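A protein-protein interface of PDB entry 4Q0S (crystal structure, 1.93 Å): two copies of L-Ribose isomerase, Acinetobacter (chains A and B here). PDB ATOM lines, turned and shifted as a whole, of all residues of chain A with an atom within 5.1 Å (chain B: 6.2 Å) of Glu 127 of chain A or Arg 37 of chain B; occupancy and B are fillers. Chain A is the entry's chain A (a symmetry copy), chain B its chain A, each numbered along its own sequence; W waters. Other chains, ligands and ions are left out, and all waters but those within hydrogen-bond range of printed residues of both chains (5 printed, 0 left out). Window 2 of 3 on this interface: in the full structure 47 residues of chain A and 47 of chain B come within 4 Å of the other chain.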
ATOM      1  N   ALA A  35       0.765 -14.091  -1.442  1.00  0.00           N
ATOM      2  CA  ALA A  35       0.976 -15.302  -0.663  1.00  0.00           C
ATOM      3  C   ALA A  35       0.950 -16.524  -1.584  1.00  0.00           C
ATOM      4  O   ALA A  35       1.692 -17.486  -1.379  1.00  0.00           O
ATOM      5  CB  ALA A  35      -0.113 -15.433   0.414  1.00  0.00           C
ATOM      6  N   LEU A  36       0.094 -16.478  -2.600  1.00  0.00           N
ATOM      7  CA  LEU A  36      -0.037 -17.585  -3.542  1.00  0.00           C
ATOM      8  C   LEU A  36       0.973 -17.455  -4.683  1.00  0.00           C
ATOM      9  O   LEU A  36       0.865 -18.125  -5.709  1.00  0.00           O
ATOM     10  CB  LEU A  36      -1.466 -17.636  -4.088  1.00  0.00           C
ATOM     11  CG  LEU A  36      -2.545 -17.887  -3.030  1.00  0.00           C
ATOM     12  CD1 LEU A  36      -3.930 -17.520  -3.591  1.00  0.00           C
ATOM     13  CD2 LEU A  36      -2.501 -19.348  -2.578  1.00  0.00           C
ATOM     14  N   SER A 125      -8.310 -19.762 -20.473  1.00  0.00           N
ATOM     15  CA  SER A 125      -7.911 -21.027 -19.865  1.00  0.00           C
ATOM     16  C   SER A 125      -7.877 -20.732 -18.367  1.00  0.00           C
ATOM     17  O   SER A 125      -7.467 -19.636 -17.959  1.00  0.00           O
ATOM     18  CB  SER A 125      -6.528 -21.478 -20.349  1.00  0.00           C
ATOM     19  OG  SER A 125      -5.488 -20.733 -19.735  1.00  0.00           O
ATOM     20  N   TYR A 126      -8.321 -21.688 -17.553  1.00  0.00           N
ATOM     21  CA  TYR A 126      -8.359 -21.486 -16.109  1.00  0.00           C
ATOM     22  C   TYR A 126      -7.485 -22.438 -15.318  1.00  0.00           C
ATOM     23  O   TYR A 126      -7.382 -23.621 -15.632  1.00  0.00           O
ATOM     24  CB  TYR A 126      -9.790 -21.630 -15.570  1.00  0.00           C
ATOM     25  CG  TYR A 126     -10.842 -20.897 -16.357  1.00  0.00           C
ATOM     26  CD1 TYR A 126     -10.709 -19.542 -16.637  1.00  0.00           C
ATOM     27  CD2 TYR A 126     -11.981 -21.562 -16.815  1.00  0.00           C
ATOM     28  CE1 TYR A 126     -11.681 -18.858 -17.353  1.00  0.00           C
ATOM     29  CE2 TYR A 126     -12.964 -20.892 -17.533  1.00  0.00           C
ATOM     30  CZ  TYR A 126     -12.808 -19.539 -17.800  1.00  0.00           C
ATOM     31  OH  TYR A 126     -13.762 -18.872 -18.531  1.00  0.00           O
ATOM     32  N   GLU A 127      -6.886 -21.904 -14.264  1.00  0.00           N
ATOM     33  CA  GLU A 127      -6.046 -22.670 -13.357  1.00  0.00           C
ATOM     34  C   GLU A 127      -6.472 -22.227 -11.959  1.00  0.00           C
ATOM     35  O   GLU A 127      -6.263 -21.076 -11.588  1.00  0.00           O
ATOM     36  CB  GLU A 127      -4.568 -22.329 -13.582  1.00  0.00           C
ATOM     37  CG  GLU A 127      -3.610 -23.053 -12.650  1.00  0.00           C
ATOM     38  CD  GLU A 127      -2.229 -22.416 -12.617  1.00  0.00           C
ATOM     39  OE1 GLU A 127      -1.683 -22.105 -13.695  1.00  0.00           O
ATOM     40  OE2 GLU A 127      -1.686 -22.240 -11.507  1.00  0.00           O
ATOM     41  N   VAL A 128      -7.095 -23.118 -11.193  1.00  0.00           N
ATOM     42  CA  VAL A 128      -7.516 -22.751  -9.848  1.00  0.00           C
ATOM     43  C   VAL A 128      -6.303 -22.805  -8.923  1.00  0.00           C
ATOM     44  O   VAL A 128      -5.573 -23.795  -8.899  1.00  0.00           O
ATOM     45  CB  VAL A 128      -8.625 -23.698  -9.317  1.00  0.00           C
ATOM     46  CG1 VAL A 128      -8.943 -23.372  -7.849  1.00  0.00           C
ATOM     47  CG2 VAL A 128      -9.891 -23.548 -10.173  1.00  0.00           C
ATOM     48  N   VAL A 129      -6.083 -21.730  -8.174  1.00  0.00           N
ATOM     49  CA  VAL A 129      -4.950 -21.662  -7.261  1.00  0.00           C
ATOM     50  C   VAL A 129      -5.399 -21.948  -5.838  1.00  0.00           C
ATOM     51  O   VAL A 129      -4.706 -22.640  -5.082  1.00  0.00           O
ATOM     52  CB  VAL A 129      -4.284 -20.271  -7.318  1.00  0.00           C
ATOM     53  CG1 VAL A 129      -3.043 -20.239  -6.418  1.00  0.00           C
ATOM     54  CG2 VAL A 129      -3.918 -19.935  -8.758  1.00  0.00           C
ATOM     55  N   LYS A 190      -5.454 -27.768 -17.049  1.00  0.00           N
ATOM     56  CA  LYS A 190      -5.868 -26.420 -17.422  1.00  0.00           C
ATOM     57  C   LYS A 190      -7.203 -26.541 -18.159  1.00  0.00           C
ATOM     58  O   LYS A 190      -7.394 -27.475 -18.935  1.00  0.00           O
ATOM     59  CB  LYS A 190      -4.826 -25.788 -18.349  1.00  0.00           C
ATOM     60  CG  LYS A 190      -3.540 -25.358 -17.658  1.00  0.00           C
ATOM     61  CD  LYS A 190      -3.654 -23.938 -17.126  1.00  0.00           C
ATOM     62  CE  LYS A 190      -2.308 -23.395 -16.677  1.00  0.00           C
ATOM     63  NZ  LYS A 190      -2.401 -21.971 -16.247  1.00  0.00           N
ATOM     64  N   VAL A 212      -9.516 -18.258  -6.011  1.00  0.00           N
ATOM     65  CA  VAL A 212      -8.416 -17.545  -6.644  1.00  0.00           C
ATOM     66  C   VAL A 212      -8.072 -18.341  -7.891  1.00  0.00           C
ATOM     67  O   VAL A 212      -7.739 -19.529  -7.810  1.00  0.00           O
ATOM     68  CB  VAL A 212      -7.172 -17.448  -5.720  1.00  0.00           C
ATOM     69  CG1 VAL A 212      -6.074 -16.611  -6.401  1.00  0.00           C
ATOM     70  CG2 VAL A 212      -7.557 -16.808  -4.402  1.00  0.00           C
ATOM     71  N   VAL A 213      -8.162 -17.688  -9.046  1.00  0.00           N
ATOM     72  CA  VAL A 213      -7.895 -18.360 -10.312  1.00  0.00           C
ATOM     73  C   VAL A 213      -6.932 -17.592 -11.196  1.00  0.00           C
ATOM     74  O   VAL A 213      -7.022 -16.374 -11.333  1.00  0.00           O
ATOM     75  CB  VAL A 213      -9.203 -18.564 -11.122  1.00  0.00           C
ATOM     76  CG1 VAL A 213      -8.919 -19.363 -12.410  1.00  0.00           C
ATOM     77  CG2 VAL A 213     -10.233 -19.285 -10.272  1.00  0.00           C
ATOM     78  N   ARG A 214      -6.011 -18.318 -11.805  1.00  0.00           N
ATOM     79  CA  ARG A 214      -5.060 -17.711 -12.708  1.00  0.00           C
ATOM     80  C   ARG A 214      -5.618 -17.888 -14.126  1.00  0.00           C
ATOM     81  O   ARG A 214      -5.883 -19.009 -14.564  1.00  0.00           O
ATOM     82  CB  ARG A 214      -3.706 -18.412 -12.563  1.00  0.00           C
ATOM     83  CG  ARG A 214      -2.602 -17.853 -13.439  1.00  0.00           C
ATOM     84  CD  ARG A 214      -1.331 -18.681 -13.277  1.00  0.00           C
ATOM     85  NE  ARG A 214      -0.616 -18.410 -12.027  1.00  0.00           N
ATOM     86  CZ  ARG A 214       0.472 -17.645 -11.949  1.00  0.00           C
ATOM     87  NH1 ARG A 214       1.067 -17.447 -10.781  1.00  0.00           N
ATOM     88  NH2 ARG A 214       0.964 -17.083 -13.048  1.00  0.00           N
ATOM     89  N   LEU B  32       8.970 -30.091  -6.766  1.00  0.00           N
ATOM     90  CA  LEU B  32       9.282 -28.690  -6.526  1.00  0.00           C
ATOM     91  C   LEU B  32       8.175 -27.848  -7.168  1.00  0.00           C
ATOM     92  O   LEU B  32       7.675 -26.885  -6.577  1.00  0.00           O
ATOM     93  CB  LEU B  32      10.647 -28.350  -7.132  1.00  0.00           C
ATOM     94  CG  LEU B  32      11.161 -26.915  -6.990  1.00  0.00           C
ATOM     95  CD1 LEU B  32      11.319 -26.553  -5.520  1.00  0.00           C
ATOM     96  CD2 LEU B  32      12.505 -26.793  -7.698  1.00  0.00           C
ATOM     97  N   GLY B  33       7.778 -28.226  -8.377  1.00  0.00           N
ATOM     98  CA  GLY B  33       6.733 -27.498  -9.066  1.00  0.00           C
ATOM     99  C   GLY B  33       5.431 -27.476  -8.288  1.00  0.00           C
ATOM    100  O   GLY B  33       4.777 -26.441  -8.184  1.00  0.00           O
ATOM    101  N   LYS B  34       5.046 -28.627  -7.749  1.00  0.00           N
ATOM    102  CA  LYS B  34       3.819 -28.726  -6.973  1.00  0.00           C
ATOM    103  C   LYS B  34       3.897 -27.846  -5.731  1.00  0.00           C
ATOM    104  O   LYS B  34       2.947 -27.133  -5.404  1.00  0.00           O
ATOM    105  CB  LYS B  34       3.562 -30.188  -6.599  1.00  0.00           C
ATOM    106  CG  LYS B  34       3.274 -31.035  -7.823  1.00  0.00           C
ATOM    107  CD  LYS B  34       2.818 -32.426  -7.470  1.00  0.00           C
ATOM    108  CE  LYS B  34       2.307 -33.134  -8.716  1.00  0.00           C
ATOM    109  NZ  LYS B  34       1.622 -34.407  -8.391  1.00  0.00           N
ATOM    110  N   ALA B  35       5.039 -27.876  -5.054  1.00  0.00           N
ATOM    111  CA  ALA B  35       5.226 -27.057  -3.865  1.00  0.00           C
ATOM    112  C   ALA B  35       4.996 -25.583  -4.208  1.00  0.00           C
ATOM    113  O   ALA B  35       4.459 -24.823  -3.401  1.00  0.00           O
ATOM    114  CB  ALA B  35       6.646 -27.252  -3.309  1.00  0.00           C
ATOM    115  N   LEU B  36       5.403 -25.187  -5.410  1.00  0.00           N
ATOM    116  CA  LEU B  36       5.254 -23.805  -5.853  1.00  0.00           C
ATOM    117  C   LEU B  36       3.883 -23.580  -6.492  1.00  0.00           C
ATOM    118  O   LEU B  36       3.648 -22.573  -7.159  1.00  0.00           O
ATOM    119  CB  LEU B  36       6.373 -23.450  -6.834  1.00  0.00           C
ATOM    120  CG  LEU B  36       7.786 -23.527  -6.246  1.00  0.00           C
ATOM    121  CD1 LEU B  36       8.828 -23.556  -7.377  1.00  0.00           C
ATOM    122  CD2 LEU B  36       8.024 -22.343  -5.306  1.00  0.00           C
ATOM    123  N   ARG B  37       2.993 -24.539  -6.273  1.00  0.00           N
ATOM    124  CA  ARG B  37       1.621 -24.502  -6.774  1.00  0.00           C
ATOM    125  C   ARG B  37       1.425 -24.524  -8.287  1.00  0.00           C
ATOM    126  O   ARG B  37       0.463 -23.940  -8.789  1.00  0.00           O
ATOM    127  CB  ARG B  37       0.868 -23.297  -6.188  1.00  0.00           C
ATOM    128  CG  ARG B  37       0.842 -23.242  -4.654  1.00  0.00           C
ATOM    129  CD  ARG B  37      -0.013 -22.065  -4.174  1.00  0.00           C
ATOM    130  NE  ARG B  37      -0.091 -21.981  -2.714  1.00  0.00           N
ATOM    131  CZ  ARG B  37      -0.817 -22.793  -1.950  1.00  0.00           C
ATOM    132  NH1 ARG B  37      -1.535 -23.760  -2.499  1.00  0.00           N
ATOM    133  NH2 ARG B  37      -0.836 -22.629  -0.637  1.00  0.00           N
ATOM    134  N   TYR B  38       2.319 -25.177  -9.024  1.00  0.00           N
ATOM    135  CA  TYR B  38       2.113 -25.272 -10.470  1.00  0.00           C
ATOM    136  C   TYR B  38       1.283 -26.557 -10.624  1.00  0.00           C
ATOM    137  O   TYR B  38       1.595 -27.579 -10.012  1.00  0.00           O
ATOM    138  CB  TYR B  38       3.439 -25.390 -11.234  1.00  0.00           C
ATOM    139  CG  TYR B  38       3.261 -25.142 -12.720  1.00  0.00           C
ATOM    140  CD1 TYR B  38       3.062 -23.847 -13.213  1.00  0.00           C
ATOM    141  CD2 TYR B  38       3.199 -26.204 -13.618  1.00  0.00           C
ATOM    142  CE1 TYR B  38       2.800 -23.621 -14.571  1.00  0.00           C
ATOM    143  CE2 TYR B  38       2.932 -25.992 -14.972  1.00  0.00           C
ATOM    144  CZ  TYR B  38       2.733 -24.699 -15.444  1.00  0.00           C
ATOM    145  OH  TYR B  38       2.452 -24.497 -16.783  1.00  0.00           O
ATOM    146  N   PRO B  39       0.215 -26.518 -11.437  1.00  0.00           N
ATOM    147  CA  PRO B  39      -0.650 -27.686 -11.643  1.00  0.00           C
ATOM    148  C   PRO B  39      -0.048 -28.796 -12.499  1.00  0.00           C
ATOM    149  O   PRO B  39      -0.404 -28.954 -13.664  1.00  0.00           O
ATOM    150  CB  PRO B  39      -1.891 -27.075 -12.284  1.00  0.00           C
ATOM    151  CG  PRO B  39      -1.291 -25.997 -13.156  1.00  0.00           C
ATOM    152  CD  PRO B  39      -0.255 -25.367 -12.233  1.00  0.00           C
ATOM    153  N   SER B  79       1.692 -27.462 -19.150  1.00  0.00           N
ATOM    154  CA  SER B  79       0.325 -27.644 -18.656  1.00  0.00           C
ATOM    155  C   SER B  79      -0.714 -27.259 -19.699  1.00  0.00           C
ATOM    156  O   SER B  79      -1.892 -27.604 -19.579  1.00  0.00           O
ATOM    157  CB  SER B  79       0.092 -26.813 -17.393  1.00  0.00           C
ATOM    158  OG  SER B  79       0.118 -25.420 -17.673  1.00  0.00           O
ATOM    159  N   ASP B 103       1.299 -22.735 -21.683  1.00  0.00           N
ATOM    160  CA  ASP B 103       1.690 -22.488 -20.296  1.00  0.00           C
ATOM    161  C   ASP B 103       2.575 -23.649 -19.864  1.00  0.00           C
ATOM    162  O   ASP B 103       2.191 -24.808 -20.005  1.00  0.00           O
ATOM    163  CB  ASP B 103       0.440 -22.432 -19.397  1.00  0.00           C
ATOM    164  CG  ASP B 103       0.710 -21.791 -18.036  1.00  0.00           C
ATOM    165  OD1 ASP B 103       1.754 -22.091 -17.424  1.00  0.00           O
ATOM    166  OD2 ASP B 103      -0.132 -20.994 -17.568  1.00  0.00           O
ATOM    167  N   ARG B 214       7.732 -19.634 -14.850  1.00  0.00           N
ATOM    168  CA  ARG B 214       6.469 -19.934 -15.486  1.00  0.00           C
ATOM    169  C   ARG B 214       6.466 -19.205 -16.836  1.00  0.00           C
ATOM    170  O   ARG B 214       6.631 -17.985 -16.895  1.00  0.00           O
ATOM    171  CB  ARG B 214       5.324 -19.439 -14.596  1.00  0.00           C
ATOM    172  CG  ARG B 214       3.934 -19.717 -15.134  1.00  0.00           C
ATOM    173  CD  ARG B 214       2.882 -19.104 -14.215  1.00  0.00           C
ATOM    174  NE  ARG B 214       2.670 -19.870 -12.983  1.00  0.00           N
ATOM    175  CZ  ARG B 214       1.636 -20.687 -12.791  1.00  0.00           C
ATOM    176  NH1 ARG B 214       1.510 -21.347 -11.647  1.00  0.00           N
ATOM    177  NH2 ARG B 214       0.728 -20.841 -13.749  1.00  0.00           N
HETATM  178  O   HOH W   1      -2.578 -24.240  -5.271  1.00  0.00           O
HETATM  179  O   HOH W   2       1.996 -20.373  -2.206  1.00  0.00           O
HETATM  180  O   HOH W   3      -4.668 -24.489  -3.147  1.00  0.00           O
HETATM  181  O   HOH W   4      -1.560 -22.082  -8.867  1.00  0.00           O
HETATM  182  O   HOH W   5      -3.104 -29.224 -17.719  1.00  0.00           O
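NH2 of Arg 214 of chain B is in salt-bridge range of OE1 of Glu 127 of chain A (2.7 Å). The side-chain amino group of Lys 190 of chain A lies within salt-bridge range of the side-chain carboxylate of Asp 103 of chain B (2.8 Å). NH2 of Arg 214 of chain B sits close to NE of Arg 214 of chain A (3.3 Å).
O of Glu 127 of chain A sits at hydrogen-bond distance from N of Arg 214 of chain A. The side-chain carboxylate (OD2) of Asp 103 of chain B lies within salt-bridge range of the guanidinium group (NH2) of Arg 214 of chain B, 3.9 Å away. The side-chain hydroxyl of Tyr 38 of chain B lies within hydrogen-bond range of the side-chain hydroxyl of Ser 79 of chain B, at 2.7 Å. The backbone carbonyl oxygen of Asp 103 of chain B is in hydrogen-bond range of the backbone NH of Ser 79 of chain B (2.8 Å). The side-chain carboxylate (OE1) of Glu 127 of chain A is in salt-bridge range of the side-chain amino group (NZ) of Lys 190 of chain A (2.7 Å). The side-chain hydroxyl (OH) of Tyr 38 of chain B lies within hydrogen-bond range of the side-chain carboxylate (OD1) of Asp 103 of chain B (2.6 Å).
Among the printed residues, merely in contact across the chains: Leu 36 of chain A with Arg 37 of chain B, Glu 127 of chain A with Arg 37 of chain B, Glu 127 of chain A with Pro 39 of chain B and Lys 190 of chain A with Ser 79 of chain B.
Of the printed residues of chain B, Leu 36 of chain A touches Arg 37 (3.6 Å). Of the printed residues of chain B, Glu 127 of chain A touches Arg 37 (3.9 Å), Pro 39 (3.5 Å) and Arg 214 (2.7 Å). Of the printed residues of chain B, Lys 190 of chain A touches Ser 79 (3.3 Å) and Asp 103 (2.8 Å). Val 213 of chain A touches none of the printed residues of chain B. Gly 33 of chain B touches none of the printed residues of chain A. Arg 37 of chain B touches just these residues of chain A: Leu 36 and Glu 127. Of the printed residues of chain A, Ser 79 of chain B touches Lys 190. Of the printed residues of chain A, Asp 103 of chain B touches Lys 190 (2.8 Å). Printed residues of chain A within 4 Å of Arg 214 of chain B: Glu 127 (2.7 Å) and Arg 214 (3.0 Å). The nearest residue of chain B that does not touch Glu 127 of chain A is Asp 103 of chain B (4.3 Å). The nearest printed residue of chain A that does not touch Arg 214 of chain B is Lys 190 of chain A (4.2 Å).
Printed residues of chain B that touch a printed residue of chain A: Arg 37, Pro 39, Ser 79, Asp 103 and Arg 214. Hydrophobic or aromatic side chains of chain B within 4 Å of the printed part of chain A: Pro 39. Of the 11 printed residues of chain A, 4 touch a printed residue of chain B. Printed residues of chain A that touch a printed residue of chain B: Leu 36, Glu 127, Lys 190 and Arg 214. Hydrophobic or aromatic side chains of chain A within 4 Å of the printed part of chain B: Leu 36. Among the printed residues, 7 pairs touch across the chains. Among the printed residues, Asp or Glu carboxylates within 4 Å of a Lys or Arg side-chain nitrogen of the other chain: Glu 127 of chain A with Arg 214 of chain B (2.7 Å) and Lys 190 of chain A with Asp 103 of chain B (2.8 Å).
Arg 214 of chain B touches its own counterpart, Arg 214 of chain A. Positions printed for both chains: 35, 36 and 214. Of the 7 pairs that touch across the chains among the printed residues, 1 has its exchanged pair printed and touching as well.
Water W4 lies within hydrogen-bond range of OE2 of Glu 127 of chain A (2.6 Å) and O of Arg 37 of chain B (2.7 Å). Water W1 lies within hydrogen-bond range of the backbone carbonyl oxygen (O) of Val 129 of chain A (2.7 Å) and the guanidinium group (NH1) of Arg 37 of chain B (3.0 Å). Water W3 lies within hydrogen-bond range of the backbone carbonyl oxygen (O) of Val 129 of chain A and the guanidinium group (NH1) of Arg 37 of chain B. Water W2 lies within hydrogen-bond range of NE of Arg 37 of chain B (2.7 Å) and O of Ala 35 of chain A (3.0 Å). Water W5 bridges the backbone carbonyl oxygen (O) of Ser 79 of chain B and the backbone NH (N) of Lys 190 of chain A.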
